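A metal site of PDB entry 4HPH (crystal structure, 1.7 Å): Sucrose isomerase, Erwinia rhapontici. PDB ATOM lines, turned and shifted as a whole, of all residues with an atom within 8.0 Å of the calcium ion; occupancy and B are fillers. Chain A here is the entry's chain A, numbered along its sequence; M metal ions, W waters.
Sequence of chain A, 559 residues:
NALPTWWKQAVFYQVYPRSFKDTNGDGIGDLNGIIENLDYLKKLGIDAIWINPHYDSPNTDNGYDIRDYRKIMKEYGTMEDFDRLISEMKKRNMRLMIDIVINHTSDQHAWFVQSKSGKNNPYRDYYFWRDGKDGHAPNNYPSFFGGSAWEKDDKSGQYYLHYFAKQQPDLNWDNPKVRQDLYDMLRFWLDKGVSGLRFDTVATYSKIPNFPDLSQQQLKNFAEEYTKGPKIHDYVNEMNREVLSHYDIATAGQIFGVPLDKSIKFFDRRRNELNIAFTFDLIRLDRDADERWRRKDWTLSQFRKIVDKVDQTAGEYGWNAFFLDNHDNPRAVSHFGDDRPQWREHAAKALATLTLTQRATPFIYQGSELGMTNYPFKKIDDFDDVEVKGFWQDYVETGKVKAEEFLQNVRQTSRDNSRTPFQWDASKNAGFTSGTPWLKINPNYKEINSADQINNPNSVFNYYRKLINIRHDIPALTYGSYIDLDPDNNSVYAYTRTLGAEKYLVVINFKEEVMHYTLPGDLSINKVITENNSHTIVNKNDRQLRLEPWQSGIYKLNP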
ATOM      1  N   PRO A  17       5.942  -7.943   1.686  1.00  0.00           N
ATOM      2  CA  PRO A  17       5.625  -7.476   0.286  1.00  0.00           C
ATOM      3  C   PRO A  17       5.666  -8.581  -0.785  1.00  0.00           C
ATOM      4  O   PRO A  17       4.841  -8.528  -1.677  1.00  0.00           O
ATOM      5  CB  PRO A  17       6.705  -6.403   0.052  1.00  0.00           C
ATOM      6  CG  PRO A  17       6.868  -5.815   1.483  1.00  0.00           C
ATOM      7  CD  PRO A  17       7.029  -7.119   2.289  1.00  0.00           C
ATOM      8  N   ARG A  18       6.583  -9.529  -0.679  1.00  0.00           N
ATOM      9  CA  ARG A  18       6.639 -10.664  -1.577  1.00  0.00           C
ATOM     10  C   ARG A  18       5.318 -11.421  -1.767  1.00  0.00           C
ATOM     11  O   ARG A  18       5.098 -12.089  -2.762  1.00  0.00           O
ATOM     12  CB  ARG A  18       7.705 -11.652  -1.033  1.00  0.00           C
ATOM     13  CG  ARG A  18       8.306 -12.616  -2.110  1.00  0.00           C
ATOM     14  CD  ARG A  18       9.410 -13.494  -1.441  1.00  0.00           C
ATOM     15  NE  ARG A  18       9.726 -14.506  -2.438  1.00  0.00           N
ATOM     16  CZ  ARG A  18      10.624 -14.309  -3.391  1.00  0.00           C
ATOM     17  NH1 ARG A  18      11.400 -13.223  -3.416  1.00  0.00           N
ATOM     18  NH2 ARG A  18      10.820 -15.274  -4.287  1.00  0.00           N
ATOM     19  N   LYS A  21       0.612  -8.317  -2.736  1.00  0.00           N
ATOM     20  CA  LYS A  21      -0.182  -8.259  -4.004  1.00  0.00           C
ATOM     21  C   LYS A  21       0.777  -8.011  -5.148  1.00  0.00           C
ATOM     22  O   LYS A  21       1.599  -7.039  -5.112  1.00  0.00           O
ATOM     23  CB  LYS A  21      -1.184  -7.039  -3.901  1.00  0.00           C
ATOM     24  CG  LYS A  21      -1.908  -6.753  -5.232  1.00  0.00           C
ATOM     25  CD  LYS A  21      -2.861  -7.932  -5.567  1.00  0.00           C
ATOM     26  CE  LYS A  21      -3.385  -7.883  -7.038  1.00  0.00           C
ATOM     27  NZ  LYS A  21      -4.584  -7.040  -7.008  1.00  0.00           N
ATOM     28  N   ASP A  22       0.677  -8.890  -6.173  1.00  0.00           N
ATOM     29  CA  ASP A  22       1.557  -8.748  -7.373  1.00  0.00           C
ATOM     30  C   ASP A  22       0.762  -7.899  -8.416  1.00  0.00           C
ATOM     31  O   ASP A  22      -0.393  -8.215  -8.756  1.00  0.00           O
ATOM     32  CB  ASP A  22       1.787 -10.153  -7.922  1.00  0.00           C
ATOM     33  CG  ASP A  22       2.540 -10.136  -9.269  1.00  0.00           C
ATOM     34  OD1 ASP A  22       3.174  -9.119  -9.602  1.00  0.00           O
ATOM     35  OD2 ASP A  22       2.398 -11.158  -9.944  1.00  0.00           O
ATOM     36  N   THR A  23       1.380  -6.857  -8.889  1.00  0.00           N
ATOM     37  CA  THR A  23       0.670  -6.020  -9.914  1.00  0.00           C
ATOM     38  C   THR A  23       1.316  -6.095 -11.286  1.00  0.00           C
ATOM     39  O   THR A  23       0.914  -5.320 -12.164  1.00  0.00           O
ATOM     40  CB  THR A  23       0.635  -4.509  -9.498  1.00  0.00           C
ATOM     41  OG1 THR A  23       1.973  -4.020  -9.293  1.00  0.00           O
ATOM     42  CG2 THR A  23      -0.208  -4.313  -8.283  1.00  0.00           C
ATOM     43  N   ASN A  24       2.313  -6.939 -11.537  1.00  0.00           N
ATOM     44  CA  ASN A  24       2.829  -6.986 -12.893  1.00  0.00           C
ATOM     45  C   ASN A  24       3.006  -8.380 -13.411  1.00  0.00           C
ATOM     46  O   ASN A  24       3.754  -8.590 -14.350  1.00  0.00           O
ATOM     47  CB  ASN A  24       4.122  -6.190 -12.993  1.00  0.00           C
ATOM     48  CG  ASN A  24       5.268  -6.842 -12.279  1.00  0.00           C
ATOM     49  OD1 ASN A  24       5.119  -7.754 -11.445  1.00  0.00           O
ATOM     50  ND2 ASN A  24       6.448  -6.422 -12.612  1.00  0.00           N
ATOM     51  N   GLY A  25       2.390  -9.350 -12.766  1.00  0.00           N
ATOM     52  CA  GLY A  25       2.381 -10.699 -13.295  1.00  0.00           C
ATOM     53  C   GLY A  25       3.586 -11.583 -13.168  1.00  0.00           C
ATOM     54  O   GLY A  25       3.602 -12.658 -13.746  1.00  0.00           O
ATOM     55  N   ASP A  26       4.610 -11.179 -12.407  1.00  0.00           N
ATOM     56  CA  ASP A  26       5.759 -12.009 -12.260  1.00  0.00           C
ATOM     57  C   ASP A  26       5.596 -13.028 -11.105  1.00  0.00           C
ATOM     58  O   ASP A  26       6.513 -13.817 -10.823  1.00  0.00           O
ATOM     59  CB  ASP A  26       7.087 -11.186 -12.207  1.00  0.00           C
ATOM     60  CG  ASP A  26       7.257 -10.419 -10.908  1.00  0.00           C
ATOM     61  OD1 ASP A  26       6.222 -10.292 -10.193  1.00  0.00           O
ATOM     62  OD2 ASP A  26       8.372  -9.930 -10.600  1.00  0.00           O
ATOM     63  N   GLY A  27       4.489 -12.922 -10.382  1.00  0.00           N
ATOM     64  CA  GLY A  27       4.180 -13.891  -9.318  1.00  0.00           C
ATOM     65  C   GLY A  27       4.714 -13.482  -7.916  1.00  0.00           C
ATOM     66  O   GLY A  27       4.604 -14.284  -6.957  1.00  0.00           O
ATOM     67  N   ILE A  28       5.335 -12.312  -7.834  1.00  0.00           N
ATOM     68  CA  ILE A  28       5.964 -11.786  -6.602  1.00  0.00           C
ATOM     69  C   ILE A  28       5.289 -10.483  -6.322  1.00  0.00           C
ATOM     70  O   ILE A  28       5.103  -9.605  -7.133  1.00  0.00           O
ATOM     71  CB  ILE A  28       7.487 -11.593  -6.758  1.00  0.00           C
ATOM     72  CG1 ILE A  28       8.135 -12.990  -7.001  1.00  0.00           C
ATOM     73  CG2 ILE A  28       8.106 -10.830  -5.585  1.00  0.00           C
ATOM     74  CD1 ILE A  28       9.555 -12.874  -7.681  1.00  0.00           C
ATOM     75  N   GLY A  29       4.846 -10.354  -5.071  1.00  0.00           N
ATOM     76  CA  GLY A  29       4.241  -9.097  -4.771  1.00  0.00           C
ATOM     77  C   GLY A  29       5.235  -7.923  -4.739  1.00  0.00           C
ATOM     78  O   GLY A  29       6.452  -8.086  -4.720  1.00  0.00           O
ATOM     79  N   ASP A  30       4.678  -6.732  -4.843  1.00  0.00           N
ATOM     80  CA  ASP A  30       5.474  -5.503  -5.073  1.00  0.00           C
ATOM     81  C   ASP A  30       4.923  -4.263  -4.379  1.00  0.00           C
ATOM     82  O   ASP A  30       3.844  -4.296  -3.784  1.00  0.00           O
ATOM     83  CB  ASP A  30       5.660  -5.321  -6.633  1.00  0.00           C
ATOM     84  CG  ASP A  30       4.336  -5.390  -7.376  1.00  0.00           C
ATOM     85  OD1 ASP A  30       3.426  -4.526  -7.081  1.00  0.00           O
ATOM     86  OD2 ASP A  30       4.148  -6.378  -8.173  1.00  0.00           O
ATOM     87  N   LEU A  31       5.720  -3.164  -4.359  1.00  0.00           N
ATOM     88  CA  LEU A  31       5.239  -1.891  -3.718  1.00  0.00           C
ATOM     89  C   LEU A  31       3.942  -1.360  -4.279  1.00  0.00           C
ATOM     90  O   LEU A  31       3.052  -0.934  -3.509  1.00  0.00           O
ATOM     91  CB  LEU A  31       6.378  -0.802  -3.720  1.00  0.00           C
ATOM     92  CG  LEU A  31       7.611  -1.270  -2.953  1.00  0.00           C
ATOM     93  CD1 LEU A  31       8.666  -0.192  -3.198  1.00  0.00           C
ATOM     94  CD2 LEU A  31       7.278  -1.478  -1.444  1.00  0.00           C
ATOM     95  N   ASN A  32       3.788  -1.322  -5.613  1.00  0.00           N
ATOM     96  CA  ASN A  32       2.481  -0.875  -6.184  1.00  0.00           C
ATOM     97  C   ASN A  32       1.278  -1.708  -5.674  1.00  0.00           C
ATOM     98  O   ASN A  32       0.176  -1.193  -5.504  1.00  0.00           O
ATOM     99  CB  ASN A  32       2.529  -0.911  -7.702  1.00  0.00           C
ATOM    100  CG  ASN A  32       3.416   0.152  -8.265  1.00  0.00           C
ATOM    101  OD1 ASN A  32       3.630   1.200  -7.630  1.00  0.00           O
ATOM    102  ND2 ASN A  32       3.938  -0.085  -9.472  1.00  0.00           N
ATOM    103  N   GLY A  33       1.547  -2.987  -5.315  1.00  0.00           N
ATOM    104  CA  GLY A  33       0.481  -3.860  -4.840  1.00  0.00           C
ATOM    105  C   GLY A  33       0.119  -3.404  -3.407  1.00  0.00           C
ATOM    106  O   GLY A  33      -1.040  -3.547  -3.014  1.00  0.00           O
ATOM    107  N   LYS A  74      14.733  -5.119  -6.742  1.00  0.00           N
ATOM    108  CA  LYS A  74      14.249  -5.018  -8.078  1.00  0.00           C
ATOM    109  C   LYS A  74      12.793  -5.554  -8.254  1.00  0.00           C
ATOM    110  O   LYS A  74      11.942  -4.926  -8.881  1.00  0.00           O
ATOM    111  CB  LYS A  74      15.230  -5.849  -8.972  1.00  0.00           C
ATOM    112  CG  LYS A  74      14.795  -6.007 -10.422  1.00  0.00           C
ATOM    113  CD  LYS A  74      14.440  -4.635 -10.996  1.00  0.00           C
ATOM    114  CE  LYS A  74      13.023  -4.580 -11.599  1.00  0.00           C
ATOM    115  NZ  LYS A  74      12.965  -4.801 -13.079  1.00  0.00           N
ATOM    116  N   GLU A  75      12.554  -6.727  -7.659  1.00  0.00           N
ATOM    117  CA  GLU A  75      11.238  -7.321  -7.670  1.00  0.00           C
ATOM    118  C   GLU A  75      10.142  -6.435  -7.063  1.00  0.00           C
ATOM    119  O   GLU A  75       8.993  -6.595  -7.391  1.00  0.00           O
ATOM    120  CB  GLU A  75      11.250  -8.684  -6.940  1.00  0.00           C
ATOM    121  CG  GLU A  75      11.975  -9.739  -7.795  1.00  0.00           C
ATOM    122  CD  GLU A  75      13.487  -9.799  -7.491  1.00  0.00           C
ATOM    123  OE1 GLU A  75      14.059  -8.898  -6.779  1.00  0.00           O
ATOM    124  OE2 GLU A  75      14.135 -10.763  -7.954  1.00  0.00           O
ATOM    125  N   TYR A  76      10.501  -5.480  -6.218  1.00  0.00           N
ATOM    126  CA  TYR A  76       9.414  -4.713  -5.525  1.00  0.00           C
ATOM    127  C   TYR A  76       9.144  -3.383  -6.194  1.00  0.00           C
ATOM    128  O   TYR A  76       8.109  -2.769  -5.963  1.00  0.00           O
ATOM    129  CB  TYR A  76       9.714  -4.432  -4.012  1.00  0.00           C
ATOM    130  CG  TYR A  76       9.775  -5.698  -3.185  1.00  0.00           C
ATOM    131  CD1 TYR A  76       9.300  -6.926  -3.657  1.00  0.00           C
ATOM    132  CD2 TYR A  76      10.230  -5.618  -1.886  1.00  0.00           C
ATOM    133  CE1 TYR A  76       9.360  -8.084  -2.835  1.00  0.00           C
ATOM    134  CE2 TYR A  76      10.315  -6.749  -1.074  1.00  0.00           C
ATOM    135  CZ  TYR A  76       9.877  -7.971  -1.571  1.00  0.00           C
ATOM    136  OH  TYR A  76       9.991  -9.075  -0.776  1.00  0.00           O
ATOM    137  N   GLY A  77      10.050  -2.919  -7.049  1.00  0.00           N
ATOM    138  CA  GLY A  77       9.742  -1.680  -7.820  1.00  0.00           C
ATOM    139  C   GLY A  77      10.955  -0.741  -7.784  1.00  0.00           C
ATOM    140  O   GLY A  77      12.112  -1.171  -7.688  1.00  0.00           O
ATOM    141  N   PHE A 432      -4.262 -12.728  -6.400  1.00  0.00           N
ATOM    142  CA  PHE A 432      -3.000 -12.200  -5.906  1.00  0.00           C
ATOM    143  C   PHE A 432      -2.117 -11.800  -7.167  1.00  0.00           C
ATOM    144  O   PHE A 432      -1.288 -10.917  -7.111  1.00  0.00           O
ATOM    145  CB  PHE A 432      -2.308 -13.301  -5.172  1.00  0.00           C
ATOM    146  CG  PHE A 432      -0.810 -13.058  -4.992  1.00  0.00           C
ATOM    147  CD1 PHE A 432      -0.361 -12.064  -4.090  1.00  0.00           C
ATOM    148  CD2 PHE A 432       0.140 -13.768  -5.727  1.00  0.00           C
ATOM    149  CE1 PHE A 432       0.989 -11.779  -3.935  1.00  0.00           C
ATOM    150  CE2 PHE A 432       1.512 -13.519  -5.530  1.00  0.00           C
ATOM    151  CZ  PHE A 432       1.973 -12.549  -4.612  1.00  0.00           C
ATOM    152  N   THR A 433      -2.234 -12.596  -8.207  1.00  0.00           N
ATOM    153  CA  THR A 433      -1.323 -12.425  -9.379  1.00  0.00           C
ATOM    154  C   THR A 433      -2.060 -12.816 -10.667  1.00  0.00           C
ATOM    155  O   THR A 433      -2.957 -13.659 -10.632  1.00  0.00           O
ATOM    156  CB  THR A 433      -0.086 -13.304  -9.269  1.00  0.00           C
ATOM    157  OG1 THR A 433       0.828 -13.018 -10.388  1.00  0.00           O
ATOM    158  CG2 THR A 433      -0.386 -14.755  -9.311  1.00  0.00           C
HETATM  159 CA    CA M   1       5.380  -8.275  -9.105  1.00  0.00          CA
HETATM  160  O   HOH W   1       7.585  -8.161  -8.608  1.00  0.00           O
HETATM  161  O   HOH W   2       6.874  -6.283  -9.529  1.00  0.00           O
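OD2 of Asp 22 lies within hydrogen-bond range of N of Gly 25, at 3.4 Å. OD2 of Asp 22 is in hydrogen-bond range of N of Gly 27 (2.8 Å). OD2 of Asp 22 sits at hydrogen-bond distance from OG1 of Thr 433. N of Asp 22 sits at hydrogen-bond distance from O of Phe 432. The side-chain carboxylate (OD1) of Asp 30 is in hydrogen-bond range of the side-chain hydroxyl (OG1) of Thr 23 (2.7 Å). The backbone NH (N) of Asp 30 sits at hydrogen-bond distance from the backbone carbonyl oxygen (O) of Lys 21 (3.1 Å). N of Gly 33 sits at hydrogen-bond distance from OD1 of Asp 30 (3.0 Å).
Water W2 bridges the backbone carbonyl oxygen (O) of Glu 75 (3.0 Å) and the side-chain amide nitrogen (ND2) of Asn 24 (3.1 Å). Water W1 bridges the backbone carbonyl oxygen of Glu 75 (2.4 Å) and the side-chain carboxylate of Asp 26 (2.8 Å).
The calcium ion is bound by water W1 (2.3 Å), the backbone carbonyl oxygen (O) of Ile 28 (2.4 Å), the side-chain amide oxygen (OD1) of Asn 24 (2.4 Å), the side-chain carboxylate (OD1) of Asp 22 (2.4 Å), the side-chain carboxylate (OD1) of Asp 26 (2.4 Å), the side-chain carboxylate (OD2) of Asp 30 (2.4 Å) and water W2 (2.5 Å). The calcium ion has seven donor atoms within binding distance.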
